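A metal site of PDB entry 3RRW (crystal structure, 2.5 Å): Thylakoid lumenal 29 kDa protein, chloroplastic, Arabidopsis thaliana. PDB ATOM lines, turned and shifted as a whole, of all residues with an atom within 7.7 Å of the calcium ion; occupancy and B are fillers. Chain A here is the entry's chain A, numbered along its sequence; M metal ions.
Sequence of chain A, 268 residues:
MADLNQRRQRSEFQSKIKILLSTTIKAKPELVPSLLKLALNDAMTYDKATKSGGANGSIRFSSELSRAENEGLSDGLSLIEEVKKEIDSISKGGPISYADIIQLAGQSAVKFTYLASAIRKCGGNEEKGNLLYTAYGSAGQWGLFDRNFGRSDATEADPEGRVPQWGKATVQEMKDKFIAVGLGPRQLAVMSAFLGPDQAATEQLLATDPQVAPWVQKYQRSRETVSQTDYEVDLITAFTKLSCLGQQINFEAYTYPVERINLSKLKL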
ATOM      1  N   LEU A  38      -0.444  12.405 -23.818  1.00  0.00           N
ATOM      2  CA  LEU A  38       0.670  11.892 -23.052  1.00  0.00           C
ATOM      3  C   LEU A  38       1.227  10.636 -23.772  1.00  0.00           C
ATOM      4  O   LEU A  38       2.448  10.498 -23.970  1.00  0.00           O
ATOM      5  CB  LEU A  38       0.185  11.558 -21.670  1.00  0.00           C
ATOM      6  CG  LEU A  38       0.923  11.909 -20.377  1.00  0.00           C
ATOM      7  CD1 LEU A  38       1.777  13.180 -20.464  1.00  0.00           C
ATOM      8  CD2 LEU A  38      -0.131  12.035 -19.266  1.00  0.00           C
ATOM      9  N   ALA A  39       0.319   9.775 -24.231  1.00  0.00           N
ATOM     10  CA  ALA A  39       0.687   8.636 -25.055  1.00  0.00           C
ATOM     11  C   ALA A  39       1.286   9.032 -26.413  1.00  0.00           C
ATOM     12  O   ALA A  39       2.264   8.423 -26.848  1.00  0.00           O
ATOM     13  CB  ALA A  39      -0.468   7.708 -25.225  1.00  0.00           C
ATOM     14  N   LEU A  40       0.759  10.081 -27.048  1.00  0.00           N
ATOM     15  CA  LEU A  40       1.304  10.575 -28.328  1.00  0.00           C
ATOM     16  C   LEU A  40       2.711  11.127 -28.163  1.00  0.00           C
ATOM     17  O   LEU A  40       3.650  10.647 -28.813  1.00  0.00           O
ATOM     18  CB  LEU A  40       0.438  11.662 -28.895  1.00  0.00           C
ATOM     19  CG  LEU A  40       0.662  12.094 -30.347  1.00  0.00           C
ATOM     20  CD1 LEU A  40       0.165  11.037 -31.223  1.00  0.00           C
ATOM     21  CD2 LEU A  40      -0.090  13.380 -30.632  1.00  0.00           C
ATOM     22  N   ASN A  41       2.851  12.129 -27.287  1.00  0.00           N
ATOM     23  CA  ASN A  41       4.135  12.787 -27.028  1.00  0.00           C
ATOM     24  C   ASN A  41       5.236  11.911 -26.435  1.00  0.00           C
ATOM     25  O   ASN A  41       6.415  12.252 -26.555  1.00  0.00           O
ATOM     26  CB  ASN A  41       3.964  14.072 -26.235  1.00  0.00           C
ATOM     27  CG  ASN A  41       3.228  15.161 -27.025  1.00  0.00           C
ATOM     28  OD1 ASN A  41       2.702  14.905 -28.109  1.00  0.00           O
ATOM     29  ND2 ASN A  41       3.238  16.381 -26.505  1.00  0.00           N
ATOM     30  N   ASP A  42       4.894  10.774 -25.853  1.00  0.00           N
ATOM     31  CA  ASP A  42       5.927   9.832 -25.370  1.00  0.00           C
ATOM     32  C   ASP A  42       6.408   9.071 -26.582  1.00  0.00           C
ATOM     33  O   ASP A  42       7.587   8.856 -26.742  1.00  0.00           O
ATOM     34  CB  ASP A  42       5.310   8.858 -24.331  1.00  0.00           C
ATOM     35  CG  ASP A  42       6.358   8.005 -23.599  1.00  0.00           C
ATOM     36  OD1 ASP A  42       7.573   8.276 -23.683  1.00  0.00           O
ATOM     37  OD2 ASP A  42       5.927   7.035 -22.908  1.00  0.00           O
ATOM     38  N   ALA A  43       5.482   8.747 -27.500  1.00  0.00           N
ATOM     39  CA  ALA A  43       5.791   7.970 -28.689  1.00  0.00           C
ATOM     40  C   ALA A  43       6.490   8.755 -29.806  1.00  0.00           C
ATOM     41  O   ALA A  43       7.367   8.221 -30.461  1.00  0.00           O
ATOM     42  CB  ALA A  43       4.552   7.328 -29.206  1.00  0.00           C
ATOM     43  N   MET A  44       6.122  10.020 -29.983  1.00  0.00           N
ATOM     44  CA  MET A  44       6.545  10.786 -31.178  1.00  0.00           C
ATOM     45  C   MET A  44       7.998  11.212 -31.213  1.00  0.00           C
ATOM     46  O   MET A  44       8.433  11.815 -32.182  1.00  0.00           O
ATOM     47  CB  MET A  44       5.654  12.010 -31.400  1.00  0.00           C
ATOM     48  CG  MET A  44       4.313  11.697 -32.009  1.00  0.00           C
ATOM     49  SD  MET A  44       4.446  10.854 -33.732  1.00  0.00           S
ATOM     50  CE  MET A  44       2.656  11.129 -34.284  1.00  0.00           C
ATOM     51  N   THR A  45       8.747  10.950 -30.163  1.00  0.00           N
ATOM     52  CA  THR A  45      10.186  11.193 -30.213  1.00  0.00           C
ATOM     53  C   THR A  45      10.911  10.110 -31.037  1.00  0.00           C
ATOM     54  O   THR A  45      12.024  10.340 -31.435  1.00  0.00           O
ATOM     55  CB  THR A  45      10.830  11.209 -28.820  1.00  0.00           C
ATOM     56  OG1 THR A  45      10.555   9.970 -28.152  1.00  0.00           O
ATOM     57  CG2 THR A  45      10.321  12.368 -28.008  1.00  0.00           C
ATOM     58  N   TYR A  46      10.298   8.953 -31.259  1.00  0.00           N
ATOM     59  CA  TYR A  46      11.000   7.912 -32.027  1.00  0.00           C
ATOM     60  C   TYR A  46      11.686   8.435 -33.308  1.00  0.00           C
ATOM     61  O   TYR A  46      11.067   9.098 -34.132  1.00  0.00           O
ATOM     62  CB  TYR A  46      10.098   6.693 -32.334  1.00  0.00           C
ATOM     63  CG  TYR A  46      10.856   5.561 -32.992  1.00  0.00           C
ATOM     64  CD1 TYR A  46      11.966   4.989 -32.377  1.00  0.00           C
ATOM     65  CD2 TYR A  46      10.485   5.063 -34.249  1.00  0.00           C
ATOM     66  CE1 TYR A  46      12.679   3.953 -32.961  1.00  0.00           C
ATOM     67  CE2 TYR A  46      11.204   4.014 -34.866  1.00  0.00           C
ATOM     68  CZ  TYR A  46      12.293   3.461 -34.203  1.00  0.00           C
ATOM     69  OH  TYR A  46      13.028   2.422 -34.785  1.00  0.00           O
ATOM     70  N   SER A  52      16.317   5.797 -31.503  1.00  0.00           N
ATOM     71  CA  SER A  52      16.168   6.337 -30.168  1.00  0.00           C
ATOM     72  C   SER A  52      14.794   6.922 -29.992  1.00  0.00           C
ATOM     73  O   SER A  52      14.107   7.196 -30.970  1.00  0.00           O
ATOM     74  CB  SER A  52      17.226   7.396 -29.911  1.00  0.00           C
ATOM     75  OG  SER A  52      16.861   8.595 -30.552  1.00  0.00           O
ATOM     76  N   GLY A  53      14.371   7.071 -28.733  1.00  0.00           N
ATOM     77  CA  GLY A  53      13.079   7.645 -28.412  1.00  0.00           C
ATOM     78  C   GLY A  53      11.945   6.652 -28.441  1.00  0.00           C
ATOM     79  O   GLY A  53      12.148   5.469 -28.269  1.00  0.00           O
ATOM     80  N   GLY A  54      10.724   7.139 -28.619  1.00  0.00           N
ATOM     81  CA  GLY A  54       9.561   6.270 -28.677  1.00  0.00           C
ATOM     82  C   GLY A  54       8.876   6.080 -27.356  1.00  0.00           C
ATOM     83  O   GLY A  54       9.201   6.746 -26.365  1.00  0.00           O
ATOM     84  N   ALA A  55       7.932   5.137 -27.356  1.00  0.00           N
ATOM     85  CA  ALA A  55       7.042   4.841 -26.244  1.00  0.00           C
ATOM     86  C   ALA A  55       7.747   4.101 -25.148  1.00  0.00           C
ATOM     87  O   ALA A  55       7.556   2.866 -25.018  1.00  0.00           O
ATOM     88  CB  ALA A  55       5.832   4.017 -26.717  1.00  0.00           C
ATOM     89  N   ASN A  56       8.437   4.862 -24.292  1.00  0.00           N
ATOM     90  CA  ASN A  56       9.385   4.342 -23.275  1.00  0.00           C
ATOM     91  C   ASN A  56       9.241   4.993 -21.891  1.00  0.00           C
ATOM     92  O   ASN A  56      10.030   4.725 -20.969  1.00  0.00           O
ATOM     93  CB  ASN A  56      10.834   4.524 -23.772  1.00  0.00           C
ATOM     94  CG  ASN A  56      11.167   5.968 -24.103  1.00  0.00           C
ATOM     95  OD1 ASN A  56      10.411   6.891 -23.763  1.00  0.00           O
ATOM     96  ND2 ASN A  56      12.292   6.178 -24.792  1.00  0.00           N
ATOM     97  N   GLY A  57       8.217   5.828 -21.738  1.00  0.00           N
ATOM     98  CA  GLY A  57       7.933   6.444 -20.441  1.00  0.00           C
ATOM     99  C   GLY A  57       8.843   7.617 -20.105  1.00  0.00           C
ATOM    100  O   GLY A  57       8.721   8.238 -19.035  1.00  0.00           O
ATOM    101  N   SER A  58       9.746   7.943 -21.017  1.00  0.00           N
ATOM    102  CA  SER A  58      10.630   9.094 -20.831  1.00  0.00           C
ATOM    103  C   SER A  58       9.869  10.362 -20.383  1.00  0.00           C
ATOM    104  O   SER A  58      10.412  11.201 -19.663  1.00  0.00           O
ATOM    105  CB  SER A  58      11.342   9.418 -22.152  1.00  0.00           C
ATOM    106  OG  SER A  58      10.384   9.807 -23.121  1.00  0.00           O
ATOM    107  N   ILE A  59       8.620  10.487 -20.840  1.00  0.00           N
ATOM    108  CA  ILE A  59       7.826  11.697 -20.654  1.00  0.00           C
ATOM    109  C   ILE A  59       7.549  12.064 -19.199  1.00  0.00           C
ATOM    110  O   ILE A  59       7.182  13.188 -18.917  1.00  0.00           O
ATOM    111  CB  ILE A  59       6.500  11.640 -21.489  1.00  0.00           C
ATOM    112  CG1 ILE A  59       5.884  13.058 -21.654  1.00  0.00           C
ATOM    113  CG2 ILE A  59       5.519  10.680 -20.900  1.00  0.00           C
ATOM    114  CD1 ILE A  59       4.961  13.182 -22.896  1.00  0.00           C
ATOM    115  N   ARG A  60       7.756  11.128 -18.287  1.00  0.00           N
ATOM    116  CA  ARG A  60       7.596  11.386 -16.844  1.00  0.00           C
ATOM    117  C   ARG A  60       8.693  12.279 -16.250  1.00  0.00           C
ATOM    118  O   ARG A  60       8.596  12.722 -15.091  1.00  0.00           O
ATOM    119  CB  ARG A  60       7.550  10.062 -16.052  1.00  0.00           C
ATOM    120  CG  ARG A  60       8.879   9.280 -16.070  1.00  0.00           C
ATOM    121  CD  ARG A  60       8.705   7.937 -15.374  1.00  0.00           C
ATOM    122  NE  ARG A  60       9.949   7.237 -15.020  1.00  0.00           N
ATOM    123  CZ  ARG A  60      10.688   6.478 -15.851  1.00  0.00           C
ATOM    124  NH1 ARG A  60      10.365   6.393 -17.153  1.00  0.00           N
ATOM    125  NH2 ARG A  60      11.778   5.839 -15.390  1.00  0.00           N
ATOM    126  N   GLU A  64      11.623  16.565 -19.574  1.00  0.00           N
ATOM    127  CA  GLU A  64      10.807  16.448 -20.780  1.00  0.00           C
ATOM    128  C   GLU A  64       9.416  17.114 -20.595  1.00  0.00           C
ATOM    129  O   GLU A  64       8.919  17.820 -21.482  1.00  0.00           O
ATOM    130  CB  GLU A  64      10.683  14.966 -21.220  1.00  0.00           C
ATOM    131  CG  GLU A  64      10.027  14.776 -22.632  1.00  0.00           C
ATOM    132  CD  GLU A  64       9.990  13.330 -23.074  1.00  0.00           C
ATOM    133  OE1 GLU A  64      10.826  12.534 -22.644  1.00  0.00           O
ATOM    134  OE2 GLU A  64       9.124  12.966 -23.852  1.00  0.00           O
ATOM    135  N   ARG A  67       8.754  20.827 -21.395  1.00  0.00           N
ATOM    136  CA  ARG A  67       8.870  21.290 -22.774  1.00  0.00           C
ATOM    137  C   ARG A  67       7.505  21.817 -23.235  1.00  0.00           C
ATOM    138  O   ARG A  67       6.463  21.323 -22.824  1.00  0.00           O
ATOM    139  CB  ARG A  67       9.448  20.192 -23.687  1.00  0.00           C
ATOM    140  CG  ARG A  67      10.658  19.483 -23.048  1.00  0.00           C
ATOM    141  CD  ARG A  67      11.735  19.160 -23.997  1.00  0.00           C
ATOM    142  NE  ARG A  67      11.625  17.821 -24.546  1.00  0.00           N
ATOM    143  CZ  ARG A  67      12.505  16.840 -24.334  1.00  0.00           C
ATOM    144  NH1 ARG A  67      13.561  17.005 -23.544  1.00  0.00           N
ATOM    145  NH2 ARG A  67      12.321  15.681 -24.929  1.00  0.00           N
ATOM    146  N   ALA A  99       6.167   3.092 -19.306  1.00  0.00           N
ATOM    147  CA  ALA A  99       5.850   3.022 -20.726  1.00  0.00           C
ATOM    148  C   ALA A  99       4.532   2.286 -21.018  1.00  0.00           C
ATOM    149  O   ALA A  99       3.785   2.696 -21.904  1.00  0.00           O
ATOM    150  CB  ALA A  99       6.985   2.399 -21.514  1.00  0.00           C
ATOM    151  N   ILE A 102       1.289   4.308 -19.440  1.00  0.00           N
ATOM    152  CA  ILE A 102       1.044   5.469 -20.301  1.00  0.00           C
ATOM    153  C   ILE A 102       0.291   5.101 -21.561  1.00  0.00           C
ATOM    154  O   ILE A 102      -0.686   5.750 -21.928  1.00  0.00           O
ATOM    155  CB  ILE A 102       2.408   6.138 -20.659  1.00  0.00           C
ATOM    156  CG1 ILE A 102       2.932   6.872 -19.413  1.00  0.00           C
ATOM    157  CG2 ILE A 102       2.269   7.030 -21.901  1.00  0.00           C
ATOM    158  CD1 ILE A 102       4.295   7.427 -19.530  1.00  0.00           C
ATOM    159  N   GLN A 103       0.703   4.012 -22.205  1.00  0.00           N
ATOM    160  CA  GLN A 103      -0.012   3.524 -23.385  1.00  0.00           C
ATOM    161  C   GLN A 103      -1.363   2.871 -23.003  1.00  0.00           C
ATOM    162  O   GLN A 103      -2.368   2.929 -23.770  1.00  0.00           O
ATOM    163  CB  GLN A 103       0.890   2.583 -24.196  1.00  0.00           C
ATOM    164  CG  GLN A 103       2.143   3.286 -24.771  1.00  0.00           C
ATOM    165  CD  GLN A 103       1.771   4.510 -25.639  1.00  0.00           C
ATOM    166  OE1 GLN A 103       0.815   4.465 -26.401  1.00  0.00           O
ATOM    167  NE2 GLN A 103       2.521   5.604 -25.471  1.00  0.00           N
ATOM    168  N   ALA A 154      12.633   3.894 -20.215  1.00  0.00           N
ATOM    169  CA  ALA A 154      13.792   4.740 -20.429  1.00  0.00           C
ATOM    170  C   ALA A 154      14.186   5.325 -19.057  1.00  0.00           C
ATOM    171  O   ALA A 154      13.355   5.436 -18.172  1.00  0.00           O
ATOM    172  CB  ALA A 154      13.467   5.838 -21.430  1.00  0.00           C
ATOM    173  N   GLU A 156      15.707   8.274 -18.695  1.00  0.00           N
ATOM    174  CA  GLU A 156      15.884   9.700 -18.833  1.00  0.00           C
ATOM    175  C   GLU A 156      15.037  10.228 -19.972  1.00  0.00           C
ATOM    176  O   GLU A 156      14.493   9.464 -20.756  1.00  0.00           O
ATOM    177  CB  GLU A 156      17.354  10.016 -19.103  1.00  0.00           C
ATOM    178  CG  GLU A 156      17.840   9.467 -20.414  1.00  0.00           C
ATOM    179  CD  GLU A 156      19.320   9.731 -20.610  1.00  0.00           C
ATOM    180  OE1 GLU A 156      20.152   8.979 -20.043  1.00  0.00           O
ATOM    181  OE2 GLU A 156      19.648  10.671 -21.349  1.00  0.00           O
ATOM    182  N   ALA A 157      14.945  11.544 -20.034  1.00  0.00           N
ATOM    183  CA  ALA A 157      14.201  12.250 -21.061  1.00  0.00           C
ATOM    184  C   ALA A 157      14.607  11.803 -22.463  1.00  0.00           C
ATOM    185  O   ALA A 157      15.704  11.288 -22.671  1.00  0.00           O
ATOM    186  CB  ALA A 157      14.441  13.718 -20.901  1.00  0.00           C
ATOM    187  N   ASP A 158      13.711  11.956 -23.434  1.00  0.00           N
ATOM    188  CA  ASP A 158      14.068  11.695 -24.815  1.00  0.00           C
ATOM    189  C   ASP A 158      14.697  12.950 -25.337  1.00  0.00           C
ATOM    190  O   ASP A 158      14.500  14.016 -24.747  1.00  0.00           O
ATOM    191  CB  ASP A 158      12.863  11.280 -25.636  1.00  0.00           C
ATOM    192  CG  ASP A 158      12.518   9.807 -25.471  1.00  0.00           C
ATOM    193  OD1 ASP A 158      13.258   9.121 -24.782  1.00  0.00           O
ATOM    194  OD2 ASP A 158      11.525   9.335 -26.023  1.00  0.00           O
ATOM    195  N   PRO A 159      15.486  12.851 -26.409  1.00  0.00           N
ATOM    196  CA  PRO A 159      16.209  14.030 -26.852  1.00  0.00           C
ATOM    197  C   PRO A 159      15.184  15.115 -27.150  1.00  0.00           C
ATOM    198  O   PRO A 159      14.055  14.778 -27.421  1.00  0.00           O
ATOM    199  CB  PRO A 159      16.901  13.550 -28.133  1.00  0.00           C
ATOM    200  CG  PRO A 159      16.933  12.037 -28.019  1.00  0.00           C
ATOM    201  CD  PRO A 159      15.628  11.725 -27.351  1.00  0.00           C
ATOM    202  N   LEU A 245       6.666   1.728 -30.735  1.00  0.00           N
ATOM    203  CA  LEU A 245       7.770   2.160 -31.570  1.00  0.00           C
ATOM    204  C   LEU A 245       9.064   2.349 -30.809  1.00  0.00           C
ATOM    205  O   LEU A 245       9.110   3.033 -29.782  1.00  0.00           O
ATOM    206  CB  LEU A 245       7.401   3.427 -32.338  1.00  0.00           C
ATOM    207  CG  LEU A 245       6.583   3.251 -33.629  1.00  0.00           C
ATOM    208  CD1 LEU A 245       6.675   4.512 -34.425  1.00  0.00           C
ATOM    209  CD2 LEU A 245       7.080   2.068 -34.453  1.00  0.00           C
HETATM  210 CA    CA M   1       9.442   8.767 -24.982  1.00  0.00          CA
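OG1 of Thr 45 sits close to O of Asp 42 (3.5 Å). The side-chain carboxylate of Asp 42 lies within hydrogen-bond range of the backbone NH of Gly 57, at 2.8 Å. The side-chain hydroxyl of Ser 58 sits close to the side-chain carboxylate of Glu 64 (2.8 Å). OD2 of Asp 158 lies close to OG1 of Thr 45, 2.4 Å away. The side-chain carboxylate (OE1) of Glu 64 lies within hydrogen-bond range of the backbone NH (N) of Asp 158, 3.0 Å away. O of Asp 158 sits at hydrogen-bond distance from NH2 of Arg 67. The backbone carbonyl oxygen (O) of Asn 56 lies within hydrogen-bond range of the backbone NH (N) of Ala 154 (2.8 Å). N of Gly 54 is in hydrogen-bond range of OG1 of Thr 45 (2.9 Å).
OG1 of Thr 45 touches the calcium ion, at 3.6 Å.
The calcium ion is bound by the side-chain carboxylate of Asp 42 (2.3 Å), the side-chain hydroxyl of Ser 58 (2.3 Å), the side-chain carboxylate of Asp 158 (2.4 Å), the side-chain amide oxygen of Asn 56 (2.4 Å), the backbone carbonyl oxygen of Gly 54 (2.5 Å) and the backbone carbonyl oxygen of Asp 42 (2.6 Å).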
